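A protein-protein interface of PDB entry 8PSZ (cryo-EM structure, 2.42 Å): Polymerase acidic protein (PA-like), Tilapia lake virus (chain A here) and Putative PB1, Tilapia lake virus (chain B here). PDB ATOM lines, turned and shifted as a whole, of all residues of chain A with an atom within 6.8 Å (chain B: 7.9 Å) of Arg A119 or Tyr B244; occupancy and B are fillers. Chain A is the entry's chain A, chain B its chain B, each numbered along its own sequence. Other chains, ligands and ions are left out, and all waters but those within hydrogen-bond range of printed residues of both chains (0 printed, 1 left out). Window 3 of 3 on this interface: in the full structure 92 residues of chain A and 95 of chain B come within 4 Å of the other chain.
The guanidinium group of Arg A119 sits at hydrogen-bond distance from the side-chain hydroxyl of Tyr B244 (3.4 Å). The backbone carbonyl oxygen of Pro A124 lies within hydrogen-bond range of the guanidinium group of Arg B247, at 3.2 Å. The side-chain carboxylate (OE2) of Glu B131 lies within salt-bridge range of the guanidinium group (NH1) of Arg A119, 2.8 Å away.
Printed residues of chain B within 4 Å of Glu A115: Leu B121 (3.5 Å). Of the printed residues of chain B, Arg A117 touches Val B240. Arg A119 touches just these residues of chain B: Leu B121 (3.3 Å), Glu B131 (2.8 Å) and Tyr B244 (3.4 Å). Glu A122 touches none of the printed residues of chain B. Printed residues of chain B within 4 Å of Leu A123: Tyr B244, Arg B247 and Arg B248. Of the printed residues of chain B, Pro A124 touches Arg B247 (3.2 Å). Of the printed residues of chain A, Leu B134 touches Leu A116 (3.9 Å). Leu B242 touches none of the printed residues of chain A. Of the printed residues of chain A, Tyr B244 touches Arg A119 (3.4 Å), Leu A120 (3.7 Å) and Leu A123 (3.999 Å). The nearest residue of chain B that does not touch Arg A119 is Arg B248 (5.6 Å). The nearest printed residue of chain A that does not touch Tyr B244 is Leu A116 (4.1 Å).
Hydrophobic or aromatic side chains of chain B that line the printed part of chain A: Leu B121, Leu B134, Leu B227, Val B240, Met B241, Ala B243 and Tyr B244. Among the printed residues, 16 pairs touch across the chains. Among the printed residues, Asp or Glu carboxylates within 4 Å of a Lys or Arg side-chain nitrogen of the other chain: Arg A119 with Glu B131 (2.8 Å).
OE2 of Glu A115 is in salt-bridge range of NH2 of Arg A119, 3.4 Å away. The side-chain hydroxyl (OH) of Tyr B244 sits close to the guanidinium group (NH1) of Arg B248 (3.4 Å). O of Leu B121 lies within hydrogen-bond range of N of Glu B131.
Glu A115 touches Leu B121. Leu A116 touches Val B240. Met B241 touches Leu A116. Val B240 touches Arg A117. Leu B227 touches Leu A120 (CD2 to CD2, 3.6 Å). CB of Ala B243 touches CD2 of Leu A120, 3.9 Å away. CA of Tyr B244 touches CD1 of Leu A120, at 3.7 Å. Arg B247 touches Leu A120. Arg B247 touches Leu A123. Leu A123 touches Arg B248 (CD1 to CG, 3.9 Å).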
ATOM      1  N   ALA A 114      -3.478 -15.854 -23.515  1.00  0.00           N
ATOM      2  CA  ALA A 114      -2.573 -15.826 -22.371  1.00  0.00           C
ATOM      3  C   ALA A 114      -1.997 -14.434 -22.157  1.00  0.00           C
ATOM      4  O   ALA A 114      -1.812 -14.001 -21.014  1.00  0.00           O
ATOM      5  CB  ALA A 114      -1.453 -16.846 -22.562  1.00  0.00           C
ATOM      6  N   GLU A 115      -1.701 -13.721 -23.244  1.00  0.00           N
ATOM      7  CA  GLU A 115      -1.168 -12.369 -23.122  1.00  0.00           C
ATOM      8  C   GLU A 115      -2.154 -11.455 -22.403  1.00  0.00           C
ATOM      9  O   GLU A 115      -1.782 -10.718 -21.482  1.00  0.00           O
ATOM     10  CB  GLU A 115      -0.835 -11.826 -24.512  1.00  0.00           C
ATOM     11  CG  GLU A 115      -0.571 -10.335 -24.558  1.00  0.00           C
ATOM     12  CD  GLU A 115       0.235  -9.932 -25.776  1.00  0.00           C
ATOM     13  OE1 GLU A 115       0.084 -10.583 -26.831  1.00  0.00           O
ATOM     14  OE2 GLU A 115       1.018  -8.964 -25.682  1.00  0.00           O
ATOM     15  N   LEU A 116      -3.427 -11.504 -22.801  1.00  0.00           N
ATOM     16  CA  LEU A 116      -4.429 -10.664 -22.155  1.00  0.00           C
ATOM     17  C   LEU A 116      -4.694 -11.106 -20.723  1.00  0.00           C
ATOM     18  O   LEU A 116      -4.952 -10.264 -19.858  1.00  0.00           O
ATOM     19  CB  LEU A 116      -5.726 -10.670 -22.963  1.00  0.00           C
ATOM     20  CG  LEU A 116      -5.721  -9.865 -24.265  1.00  0.00           C
ATOM     21  CD1 LEU A 116      -7.100  -9.877 -24.895  1.00  0.00           C
ATOM     22  CD2 LEU A 116      -5.252  -8.434 -24.039  1.00  0.00           C
ATOM     23  N   ARG A 117      -4.634 -12.409 -20.448  1.00  0.00           N
ATOM     24  CA  ARG A 117      -4.793 -12.864 -19.071  1.00  0.00           C
ATOM     25  C   ARG A 117      -3.661 -12.349 -18.190  1.00  0.00           C
ATOM     26  O   ARG A 117      -3.892 -11.924 -17.053  1.00  0.00           O
ATOM     27  CB  ARG A 117      -4.863 -14.388 -19.025  1.00  0.00           C
ATOM     28  CG  ARG A 117      -6.269 -14.935 -19.186  1.00  0.00           C
ATOM     29  CD  ARG A 117      -6.276 -16.448 -19.205  1.00  0.00           C
ATOM     30  NE  ARG A 117      -7.513 -16.986 -19.757  1.00  0.00           N
ATOM     31  CZ  ARG A 117      -8.672 -17.016 -19.115  1.00  0.00           C
ATOM     32  NH1 ARG A 117      -8.799 -16.528 -17.891  1.00  0.00           N
ATOM     33  NH2 ARG A 117      -9.732 -17.548 -19.715  1.00  0.00           N
ATOM     34  N   GLU A 118      -2.428 -12.370 -18.701  1.00  0.00           N
ATOM     35  CA  GLU A 118      -1.308 -11.810 -17.951  1.00  0.00           C
ATOM     36  C   GLU A 118      -1.488 -10.311 -17.736  1.00  0.00           C
ATOM     37  O   GLU A 118      -1.263  -9.802 -16.630  1.00  0.00           O
ATOM     38  CB  GLU A 118       0.003 -12.095 -18.686  1.00  0.00           C
ATOM     39  CG  GLU A 118       1.232 -11.519 -18.012  1.00  0.00           C
ATOM     40  CD  GLU A 118       2.524 -11.990 -18.650  1.00  0.00           C
ATOM     41  OE1 GLU A 118       2.470 -12.552 -19.765  1.00  0.00           O
ATOM     42  OE2 GLU A 118       3.596 -11.798 -18.038  1.00  0.00           O
ATOM     43  N   ARG A 119      -1.907  -9.592 -18.779  1.00  0.00           N
ATOM     44  CA  ARG A 119      -2.165  -8.163 -18.632  1.00  0.00           C
ATOM     45  C   ARG A 119      -3.196  -7.905 -17.543  1.00  0.00           C
ATOM     46  O   ARG A 119      -3.021  -7.009 -16.709  1.00  0.00           O
ATOM     47  CB  ARG A 119      -2.643  -7.578 -19.958  1.00  0.00           C
ATOM     48  CG  ARG A 119      -1.582  -7.518 -21.032  1.00  0.00           C
ATOM     49  CD  ARG A 119      -1.854  -6.385 -21.992  1.00  0.00           C
ATOM     50  NE  ARG A 119      -1.231  -6.607 -23.290  1.00  0.00           N
ATOM     51  CZ  ARG A 119      -1.517  -5.917 -24.385  1.00  0.00           C
ATOM     52  NH1 ARG A 119      -2.424  -4.955 -24.377  1.00  0.00           N
ATOM     53  NH2 ARG A 119      -0.875  -6.198 -25.514  1.00  0.00           N
ATOM     54  N   LEU A 120      -4.278  -8.684 -17.536  1.00  0.00           N
ATOM     55  CA  LEU A 120      -5.298  -8.531 -16.505  1.00  0.00           C
ATOM     56  C   LEU A 120      -4.726  -8.833 -15.128  1.00  0.00           C
ATOM     57  O   LEU A 120      -5.059  -8.159 -14.146  1.00  0.00           O
ATOM     58  CB  LEU A 120      -6.484  -9.447 -16.813  1.00  0.00           C
ATOM     59  CG  LEU A 120      -7.906  -8.984 -16.477  1.00  0.00           C
ATOM     60  CD1 LEU A 120      -8.143  -7.523 -16.820  1.00  0.00           C
ATOM     61  CD2 LEU A 120      -8.907  -9.862 -17.207  1.00  0.00           C
ATOM     62  N   LEU A 121      -3.861  -9.844 -15.036  1.00  0.00           N
ATOM     63  CA  LEU A 121      -3.257 -10.186 -13.754  1.00  0.00           C
ATOM     64  C   LEU A 121      -2.417  -9.037 -13.212  1.00  0.00           C
ATOM     65  O   LEU A 121      -2.424  -8.772 -12.004  1.00  0.00           O
ATOM     66  CB  LEU A 121      -2.407 -11.448 -13.898  1.00  0.00           C
ATOM     67  CG  LEU A 121      -2.028 -12.144 -12.590  1.00  0.00           C
ATOM     68  CD1 LEU A 121      -3.249 -12.762 -11.927  1.00  0.00           C
ATOM     69  CD2 LEU A 121      -0.959 -13.194 -12.839  1.00  0.00           C
ATOM     70  N   GLU A 122      -1.679  -8.346 -14.083  1.00  0.00           N
ATOM     71  CA  GLU A 122      -0.839  -7.247 -13.613  1.00  0.00           C
ATOM     72  C   GLU A 122      -1.634  -6.004 -13.232  1.00  0.00           C
ATOM     73  O   GLU A 122      -1.062  -5.094 -12.624  1.00  0.00           O
ATOM     74  CB  GLU A 122       0.196  -6.865 -14.676  1.00  0.00           C
ATOM     75  CG  GLU A 122       1.026  -8.020 -15.225  1.00  0.00           C
ATOM     76  CD  GLU A 122       1.622  -8.908 -14.147  1.00  0.00           C
ATOM     77  OE1 GLU A 122       1.684  -8.483 -12.975  1.00  0.00           O
ATOM     78  OE2 GLU A 122       2.034 -10.040 -14.476  1.00  0.00           O
ATOM     79  N   LEU A 123      -2.918  -5.935 -13.567  1.00  0.00           N
ATOM     80  CA  LEU A 123      -3.719  -4.760 -13.264  1.00  0.00           C
ATOM     81  C   LEU A 123      -4.282  -4.839 -11.847  1.00  0.00           C
ATOM     82  O   LEU A 123      -4.270  -5.900 -11.221  1.00  0.00           O
ATOM     83  CB  LEU A 123      -4.843  -4.620 -14.286  1.00  0.00           C
ATOM     84  CG  LEU A 123      -4.389  -4.129 -15.663  1.00  0.00           C
ATOM     85  CD1 LEU A 123      -5.452  -4.397 -16.711  1.00  0.00           C
ATOM     86  CD2 LEU A 123      -4.039  -2.650 -15.626  1.00  0.00           C
ATOM     87  N   PRO A 124      -4.771  -3.719 -11.311  1.00  0.00           N
ATOM     88  CA  PRO A 124      -5.225  -3.712  -9.913  1.00  0.00           C
ATOM     89  C   PRO A 124      -6.391  -4.661  -9.678  1.00  0.00           C
ATOM     90  O   PRO A 124      -7.217  -4.902 -10.559  1.00  0.00           O
ATOM     91  CB  PRO A 124      -5.640  -2.254  -9.678  1.00  0.00           C
ATOM     92  CG  PRO A 124      -5.005  -1.476 -10.771  1.00  0.00           C
ATOM     93  CD  PRO A 124      -4.902  -2.395 -11.937  1.00  0.00           C
ATOM     94  N   LEU B 121      -2.090  -9.427 -31.595  1.00  0.00           N
ATOM     95  CA  LEU B 121      -2.882  -8.250 -31.260  1.00  0.00           C
ATOM     96  C   LEU B 121      -2.610  -7.090 -32.207  1.00  0.00           C
ATOM     97  O   LEU B 121      -3.450  -6.193 -32.326  1.00  0.00           O
ATOM     98  CB  LEU B 121      -2.607  -7.818 -29.820  1.00  0.00           C
ATOM     99  CG  LEU B 121      -3.207  -8.705 -28.729  1.00  0.00           C
ATOM    100  CD1 LEU B 121      -2.570  -8.393 -27.387  1.00  0.00           C
ATOM    101  CD2 LEU B 121      -4.714  -8.536 -28.658  1.00  0.00           C
ATOM    102  N   SER B 122      -1.463  -7.089 -32.881  1.00  0.00           N
ATOM    103  CA  SER B 122      -1.120  -6.042 -33.831  1.00  0.00           C
ATOM    104  C   SER B 122      -1.568  -6.352 -35.253  1.00  0.00           C
ATOM    105  O   SER B 122      -1.576  -5.446 -36.093  1.00  0.00           O
ATOM    106  CB  SER B 122       0.393  -5.798 -33.819  1.00  0.00           C
ATOM    107  OG  SER B 122       1.096  -6.981 -33.484  1.00  0.00           O
ATOM    108  N   VAL B 130      -6.891  -5.839 -33.151  1.00  0.00           N
ATOM    109  CA  VAL B 130      -7.513  -6.223 -31.887  1.00  0.00           C
ATOM    110  C   VAL B 130      -7.018  -5.324 -30.762  1.00  0.00           C
ATOM    111  O   VAL B 130      -7.785  -4.947 -29.869  1.00  0.00           O
ATOM    112  CB  VAL B 130      -7.249  -7.708 -31.583  1.00  0.00           C
ATOM    113  CG1 VAL B 130      -7.901  -8.105 -30.270  1.00  0.00           C
ATOM    114  CG2 VAL B 130      -7.762  -8.580 -32.714  1.00  0.00           C
ATOM    115  N   GLU B 131      -5.732  -4.968 -30.783  1.00  0.00           N
ATOM    116  CA  GLU B 131      -5.207  -4.055 -29.773  1.00  0.00           C
ATOM    117  C   GLU B 131      -5.945  -2.723 -29.812  1.00  0.00           C
ATOM    118  O   GLU B 131      -6.372  -2.202 -28.774  1.00  0.00           O
ATOM    119  CB  GLU B 131      -3.706  -3.848 -29.990  1.00  0.00           C
ATOM    120  CG  GLU B 131      -3.014  -3.040 -28.897  1.00  0.00           C
ATOM    121  CD  GLU B 131      -2.693  -3.868 -27.667  1.00  0.00           C
ATOM    122  OE1 GLU B 131      -1.675  -4.590 -27.683  1.00  0.00           O
ATOM    123  OE2 GLU B 131      -3.456  -3.794 -26.681  1.00  0.00           O
ATOM    124  N   LEU B 134      -9.590  -3.097 -28.581  1.00  0.00           N
ATOM    125  CA  LEU B 134      -9.640  -3.144 -27.125  1.00  0.00           C
ATOM    126  C   LEU B 134      -9.381  -1.770 -26.522  1.00  0.00           C
ATOM    127  O   LEU B 134     -10.011  -1.390 -25.529  1.00  0.00           O
ATOM    128  CB  LEU B 134      -8.624  -4.159 -26.600  1.00  0.00           C
ATOM    129  CG  LEU B 134      -8.871  -5.616 -26.998  1.00  0.00           C
ATOM    130  CD1 LEU B 134      -7.650  -6.465 -26.689  1.00  0.00           C
ATOM    131  CD2 LEU B 134     -10.102  -6.165 -26.297  1.00  0.00           C
ATOM    132  N   SER B 135      -8.449  -1.013 -27.104  1.00  0.00           N
ATOM    133  CA  SER B 135      -8.173   0.327 -26.599  1.00  0.00           C
ATOM    134  C   SER B 135      -9.392   1.233 -26.735  1.00  0.00           C
ATOM    135  O   SER B 135      -9.726   1.980 -25.810  1.00  0.00           O
ATOM    136  CB  SER B 135      -6.975   0.923 -27.336  1.00  0.00           C
ATOM    137  OG  SER B 135      -6.943   2.332 -27.209  1.00  0.00           O
ATOM    138  N   ARG B 138     -12.987   0.446 -24.488  1.00  0.00           N
ATOM    139  CA  ARG B 138     -13.050   0.704 -23.058  1.00  0.00           C
ATOM    140  C   ARG B 138     -13.491   2.125 -22.730  1.00  0.00           C
ATOM    141  O   ARG B 138     -13.530   2.487 -21.552  1.00  0.00           O
ATOM    142  CB  ARG B 138     -11.687   0.431 -22.420  1.00  0.00           C
ATOM    143  CG  ARG B 138     -10.723   1.601 -22.509  1.00  0.00           C
ATOM    144  CD  ARG B 138      -9.285   1.144 -22.415  1.00  0.00           C
ATOM    145  NE  ARG B 138      -8.388   2.032 -23.146  1.00  0.00           N
ATOM    146  CZ  ARG B 138      -7.509   2.854 -22.589  1.00  0.00           C
ATOM    147  NH1 ARG B 138      -7.378   2.949 -21.275  1.00  0.00           N
ATOM    148  NH2 ARG B 138      -6.739   3.602 -23.373  1.00  0.00           N
ATOM    149  N   PHE B 164     -17.601  -3.051 -27.662  1.00  0.00           N
ATOM    150  CA  PHE B 164     -18.018  -3.486 -26.336  1.00  0.00           C
ATOM    151  C   PHE B 164     -19.421  -4.073 -26.376  1.00  0.00           C
ATOM    152  O   PHE B 164     -19.675  -5.131 -25.790  1.00  0.00           O
ATOM    153  CB  PHE B 164     -17.950  -2.300 -25.373  1.00  0.00           C
ATOM    154  CG  PHE B 164     -18.061  -2.677 -23.925  1.00  0.00           C
ATOM    155  CD1 PHE B 164     -16.942  -3.061 -23.208  1.00  0.00           C
ATOM    156  CD2 PHE B 164     -19.282  -2.635 -23.277  1.00  0.00           C
ATOM    157  CE1 PHE B 164     -17.042  -3.402 -21.875  1.00  0.00           C
ATOM    158  CE2 PHE B 164     -19.387  -2.975 -21.946  1.00  0.00           C
ATOM    159  CZ  PHE B 164     -18.266  -3.358 -21.244  1.00  0.00           C
ATOM    160  N   ALA B 223     -14.525  -6.700 -12.489  1.00  0.00           N
ATOM    161  CA  ALA B 223     -14.078  -7.419 -13.675  1.00  0.00           C
ATOM    162  C   ALA B 223     -13.641  -8.837 -13.334  1.00  0.00           C
ATOM    163  O   ALA B 223     -13.830  -9.754 -14.141  1.00  0.00           O
ATOM    164  CB  ALA B 223     -12.934  -6.661 -14.345  1.00  0.00           C
ATOM    165  N   LEU B 227     -15.156 -12.152 -15.111  1.00  0.00           N
ATOM    166  CA  LEU B 227     -14.299 -13.149 -15.741  1.00  0.00           C
ATOM    167  C   LEU B 227     -14.471 -14.511 -15.089  1.00  0.00           C
ATOM    168  O   LEU B 227     -14.431 -15.536 -15.772  1.00  0.00           O
ATOM    169  CB  LEU B 227     -12.837 -12.704 -15.677  1.00  0.00           C
ATOM    170  CG  LEU B 227     -11.842 -13.549 -16.480  1.00  0.00           C
ATOM    171  CD1 LEU B 227     -12.228 -13.614 -17.952  1.00  0.00           C
ATOM    172  CD2 LEU B 227     -10.434 -13.006 -16.323  1.00  0.00           C
ATOM    173  N   TRP B 230     -17.696 -15.907 -16.532  1.00  0.00           N
ATOM    174  CA  TRP B 230     -17.564 -16.193 -17.956  1.00  0.00           C
ATOM    175  C   TRP B 230     -16.663 -17.396 -18.203  1.00  0.00           C
ATOM    176  O   TRP B 230     -16.921 -18.196 -19.110  1.00  0.00           O
ATOM    177  CB  TRP B 230     -17.039 -14.956 -18.684  1.00  0.00           C
ATOM    178  CG  TRP B 230     -18.025 -13.825 -18.703  1.00  0.00           C
ATOM    179  CD1 TRP B 230     -19.383 -13.923 -18.629  1.00  0.00           C
ATOM    180  CD2 TRP B 230     -17.730 -12.426 -18.793  1.00  0.00           C
ATOM    181  NE1 TRP B 230     -19.952 -12.678 -18.670  1.00  0.00           N
ATOM    182  CE2 TRP B 230     -18.960 -11.740 -18.770  1.00  0.00           C
ATOM    183  CE3 TRP B 230     -16.548 -11.688 -18.890  1.00  0.00           C
ATOM    184  CZ2 TRP B 230     -19.041 -10.352 -18.843  1.00  0.00           C
ATOM    185  CZ3 TRP B 230     -16.631 -10.311 -18.961  1.00  0.00           C
ATOM    186  CH2 TRP B 230     -17.869  -9.657 -18.939  1.00  0.00           C
ATOM    187  N   SER B 237     -12.007 -16.494 -25.084  1.00  0.00           N
ATOM    188  CA  SER B 237     -11.313 -15.252 -25.396  1.00  0.00           C
ATOM    189  C   SER B 237     -12.262 -14.065 -25.443  1.00  0.00           C
ATOM    190  O   SER B 237     -11.854 -12.945 -25.135  1.00  0.00           O
ATOM    191  CB  SER B 237     -10.571 -15.385 -26.725  1.00  0.00           C
ATOM    192  OG  SER B 237      -9.275 -15.914 -26.526  1.00  0.00           O
ATOM    193  N   ILE B 238     -13.520 -14.279 -25.829  1.00  0.00           N
ATOM    194  CA  ILE B 238     -14.491 -13.189 -25.790  1.00  0.00           C
ATOM    195  C   ILE B 238     -14.656 -12.689 -24.361  1.00  0.00           C
ATOM    196  O   ILE B 238     -14.636 -11.480 -24.097  1.00  0.00           O
ATOM    197  CB  ILE B 238     -15.836 -13.643 -26.389  1.00  0.00           C
ATOM    198  CG1 ILE B 238     -15.698 -13.871 -27.896  1.00  0.00           C
ATOM    199  CG2 ILE B 238     -16.918 -12.611 -26.105  1.00  0.00           C
ATOM    200  CD1 ILE B 238     -16.837 -14.669 -28.498  1.00  0.00           C
ATOM    201  N   GLY B 239     -14.809 -13.617 -23.417  1.00  0.00           N
ATOM    202  CA  GLY B 239     -14.917 -13.227 -22.022  1.00  0.00           C
ATOM    203  C   GLY B 239     -13.661 -12.551 -21.514  1.00  0.00           C
ATOM    204  O   GLY B 239     -13.731 -11.563 -20.778  1.00  0.00           O
ATOM    205  N   VAL B 240     -12.493 -13.065 -21.904  1.00  0.00           N
ATOM    206  CA  VAL B 240     -11.237 -12.456 -21.471  1.00  0.00           C
ATOM    207  C   VAL B 240     -11.132 -11.026 -21.991  1.00  0.00           C
ATOM    208  O   VAL B 240     -10.766 -10.103 -21.254  1.00  0.00           O
ATOM    209  CB  VAL B 240     -10.040 -13.312 -21.927  1.00  0.00           C
ATOM    210  CG1 VAL B 240      -8.736 -12.540 -21.772  1.00  0.00           C
ATOM    211  CG2 VAL B 240      -9.996 -14.612 -21.143  1.00  0.00           C
ATOM    212  N   MET B 241     -11.453 -10.823 -23.269  1.00  0.00           N
ATOM    213  CA  MET B 241     -11.375  -9.492 -23.861  1.00  0.00           C
ATOM    214  C   MET B 241     -12.350  -8.535 -23.191  1.00  0.00           C
ATOM    215  O   MET B 241     -12.008  -7.380 -22.908  1.00  0.00           O
ATOM    216  CB  MET B 241     -11.665  -9.574 -25.358  1.00  0.00           C
ATOM    217  CG  MET B 241     -10.438  -9.790 -26.222  1.00  0.00           C
ATOM    218  SD  MET B 241     -10.777  -9.531 -27.970  1.00  0.00           S
ATOM    219  CE  MET B 241     -11.751 -10.986 -28.335  1.00  0.00           C
ATOM    220  N   LEU B 242     -13.576  -8.997 -22.937  1.00  0.00           N
ATOM    221  CA  LEU B 242     -14.562  -8.141 -22.293  1.00  0.00           C
ATOM    222  C   LEU B 242     -14.125  -7.765 -20.883  1.00  0.00           C
ATOM    223  O   LEU B 242     -14.256  -6.607 -20.473  1.00  0.00           O
ATOM    224  CB  LEU B 242     -15.918  -8.846 -22.274  1.00  0.00           C
ATOM    225  CG  LEU B 242     -17.199  -8.009 -22.306  1.00  0.00           C
ATOM    226  CD1 LEU B 242     -17.115  -6.833 -23.267  1.00  0.00           C
ATOM    227  CD2 LEU B 242     -18.356  -8.908 -22.680  1.00  0.00           C
ATOM    228  N   ALA B 243     -13.597  -8.731 -20.125  1.00  0.00           N
ATOM    229  CA  ALA B 243     -13.120  -8.434 -18.779  1.00  0.00           C
ATOM    230  C   ALA B 243     -11.954  -7.457 -18.816  1.00  0.00           C
ATOM    231  O   ALA B 243     -11.855  -6.562 -17.969  1.00  0.00           O
ATOM    232  CB  ALA B 243     -12.715  -9.726 -18.071  1.00  0.00           C
ATOM    233  N   TYR B 244     -11.058  -7.616 -19.792  1.00  0.00           N
ATOM    234  CA  TYR B 244      -9.941  -6.691 -19.932  1.00  0.00           C
ATOM    235  C   TYR B 244     -10.430  -5.278 -20.219  1.00  0.00           C
ATOM    236  O   TYR B 244      -9.919  -4.309 -19.649  1.00  0.00           O
ATOM    237  CB  TYR B 244      -9.013  -7.176 -21.045  1.00  0.00           C
ATOM    238  CG  TYR B 244      -7.800  -6.307 -21.271  1.00  0.00           C
ATOM    239  CD1 TYR B 244      -6.765  -6.272 -20.349  1.00  0.00           C
ATOM    240  CD2 TYR B 244      -7.684  -5.531 -22.414  1.00  0.00           C
ATOM    241  CE1 TYR B 244      -5.655  -5.483 -20.554  1.00  0.00           C
ATOM    242  CE2 TYR B 244      -6.576  -4.741 -22.630  1.00  0.00           C
ATOM    243  CZ  TYR B 244      -5.564  -4.722 -21.696  1.00  0.00           C
ATOM    244  OH  TYR B 244      -4.458  -3.935 -21.906  1.00  0.00           O
ATOM    245  N   MET B 245     -11.417  -5.140 -21.104  1.00  0.00           N
ATOM    246  CA  MET B 245     -11.948  -3.815 -21.404  1.00  0.00           C
ATOM    247  C   MET B 245     -12.670  -3.226 -20.197  1.00  0.00           C
ATOM    248  O   MET B 245     -12.632  -2.011 -19.976  1.00  0.00           O
ATOM    249  CB  MET B 245     -12.884  -3.881 -22.610  1.00  0.00           C
ATOM    250  CG  MET B 245     -12.190  -3.578 -23.931  1.00  0.00           C
ATOM    251  SD  MET B 245     -13.225  -3.714 -25.407  1.00  0.00           S
ATOM    252  CE  MET B 245     -14.277  -5.106 -25.014  1.00  0.00           C
ATOM    253  N   VAL B 246     -13.336  -4.068 -19.406  1.00  0.00           N
ATOM    254  CA  VAL B 246     -14.019  -3.576 -18.214  1.00  0.00           C
ATOM    255  C   VAL B 246     -13.011  -3.084 -17.183  1.00  0.00           C
ATOM    256  O   VAL B 246     -13.221  -2.055 -16.530  1.00  0.00           O
ATOM    257  CB  VAL B 246     -14.935  -4.669 -17.633  1.00  0.00           C
ATOM    258  CG1 VAL B 246     -15.412  -4.284 -16.243  1.00  0.00           C
ATOM    259  CG2 VAL B 246     -16.119  -4.909 -18.552  1.00  0.00           C
ATOM    260  N   ARG B 247     -11.904  -3.810 -17.014  1.00  0.00           N
ATOM    261  CA  ARG B 247     -10.898  -3.402 -16.039  1.00  0.00           C
ATOM    262  C   ARG B 247     -10.276  -2.059 -16.400  1.00  0.00           C
ATOM    263  O   ARG B 247      -9.928  -1.278 -15.508  1.00  0.00           O
ATOM    264  CB  ARG B 247      -9.816  -4.477 -15.927  1.00  0.00           C
ATOM    265  CG  ARG B 247      -8.639  -4.109 -15.029  1.00  0.00           C
ATOM    266  CD  ARG B 247      -9.054  -3.929 -13.578  1.00  0.00           C
ATOM    267  NE  ARG B 247      -9.311  -5.209 -12.927  1.00  0.00           N
ATOM    268  CZ  ARG B 247     -10.166  -5.394 -11.931  1.00  0.00           C
ATOM    269  NH1 ARG B 247     -10.882  -4.398 -11.436  1.00  0.00           N
ATOM    270  NH2 ARG B 247     -10.302  -6.611 -11.415  1.00  0.00           N
ATOM    271  N   ARG B 248     -10.127  -1.772 -17.692  1.00  0.00           N
ATOM    272  CA  ARG B 248      -9.431  -0.585 -18.164  1.00  0.00           C
ATOM    273  C   ARG B 248     -10.383   0.524 -18.598  1.00  0.00           C
ATOM    274  O   ARG B 248      -9.956   1.469 -19.268  1.00  0.00           O
ATOM    275  CB  ARG B 248      -8.502  -0.957 -19.318  1.00  0.00           C
ATOM    276  CG  ARG B 248      -7.227  -1.638 -18.877  1.00  0.00           C
ATOM    277  CD  ARG B 248      -6.403  -2.062 -20.068  1.00  0.00           C
ATOM    278  NE  ARG B 248      -5.683  -0.940 -20.662  1.00  0.00           N
ATOM    279  CZ  ARG B 248      -5.711  -0.609 -21.947  1.00  0.00           C
ATOM    280  NH1 ARG B 248      -6.418  -1.299 -22.829  1.00  0.00           N
ATOM    281  NH2 ARG B 248      -5.012   0.444 -22.359  1.00  0.00           N
ATOM    282  N   LYS B 249     -11.655   0.436 -18.224  1.00  0.00           N
ATOM    283  CA  LYS B 249     -12.640   1.388 -18.717  1.00  0.00           C
ATOM    284  C   LYS B 249     -12.312   2.805 -18.262  1.00  0.00           C
ATOM    285  O   LYS B 249     -11.815   3.024 -17.153  1.00  0.00           O
ATOM    286  CB  LYS B 249     -14.039   0.994 -18.243  1.00  0.00           C
ATOM    287  CG  LYS B 249     -14.247   1.111 -16.744  1.00  0.00           C
ATOM    288  CD  LYS B 249     -15.693   0.877 -16.363  1.00  0.00           C
ATOM    289  CE  LYS B 249     -15.874  -0.421 -15.607  1.00  0.00           C
ATOM    290  NZ  LYS B 249     -15.102  -0.451 -14.340  1.00  0.00           N
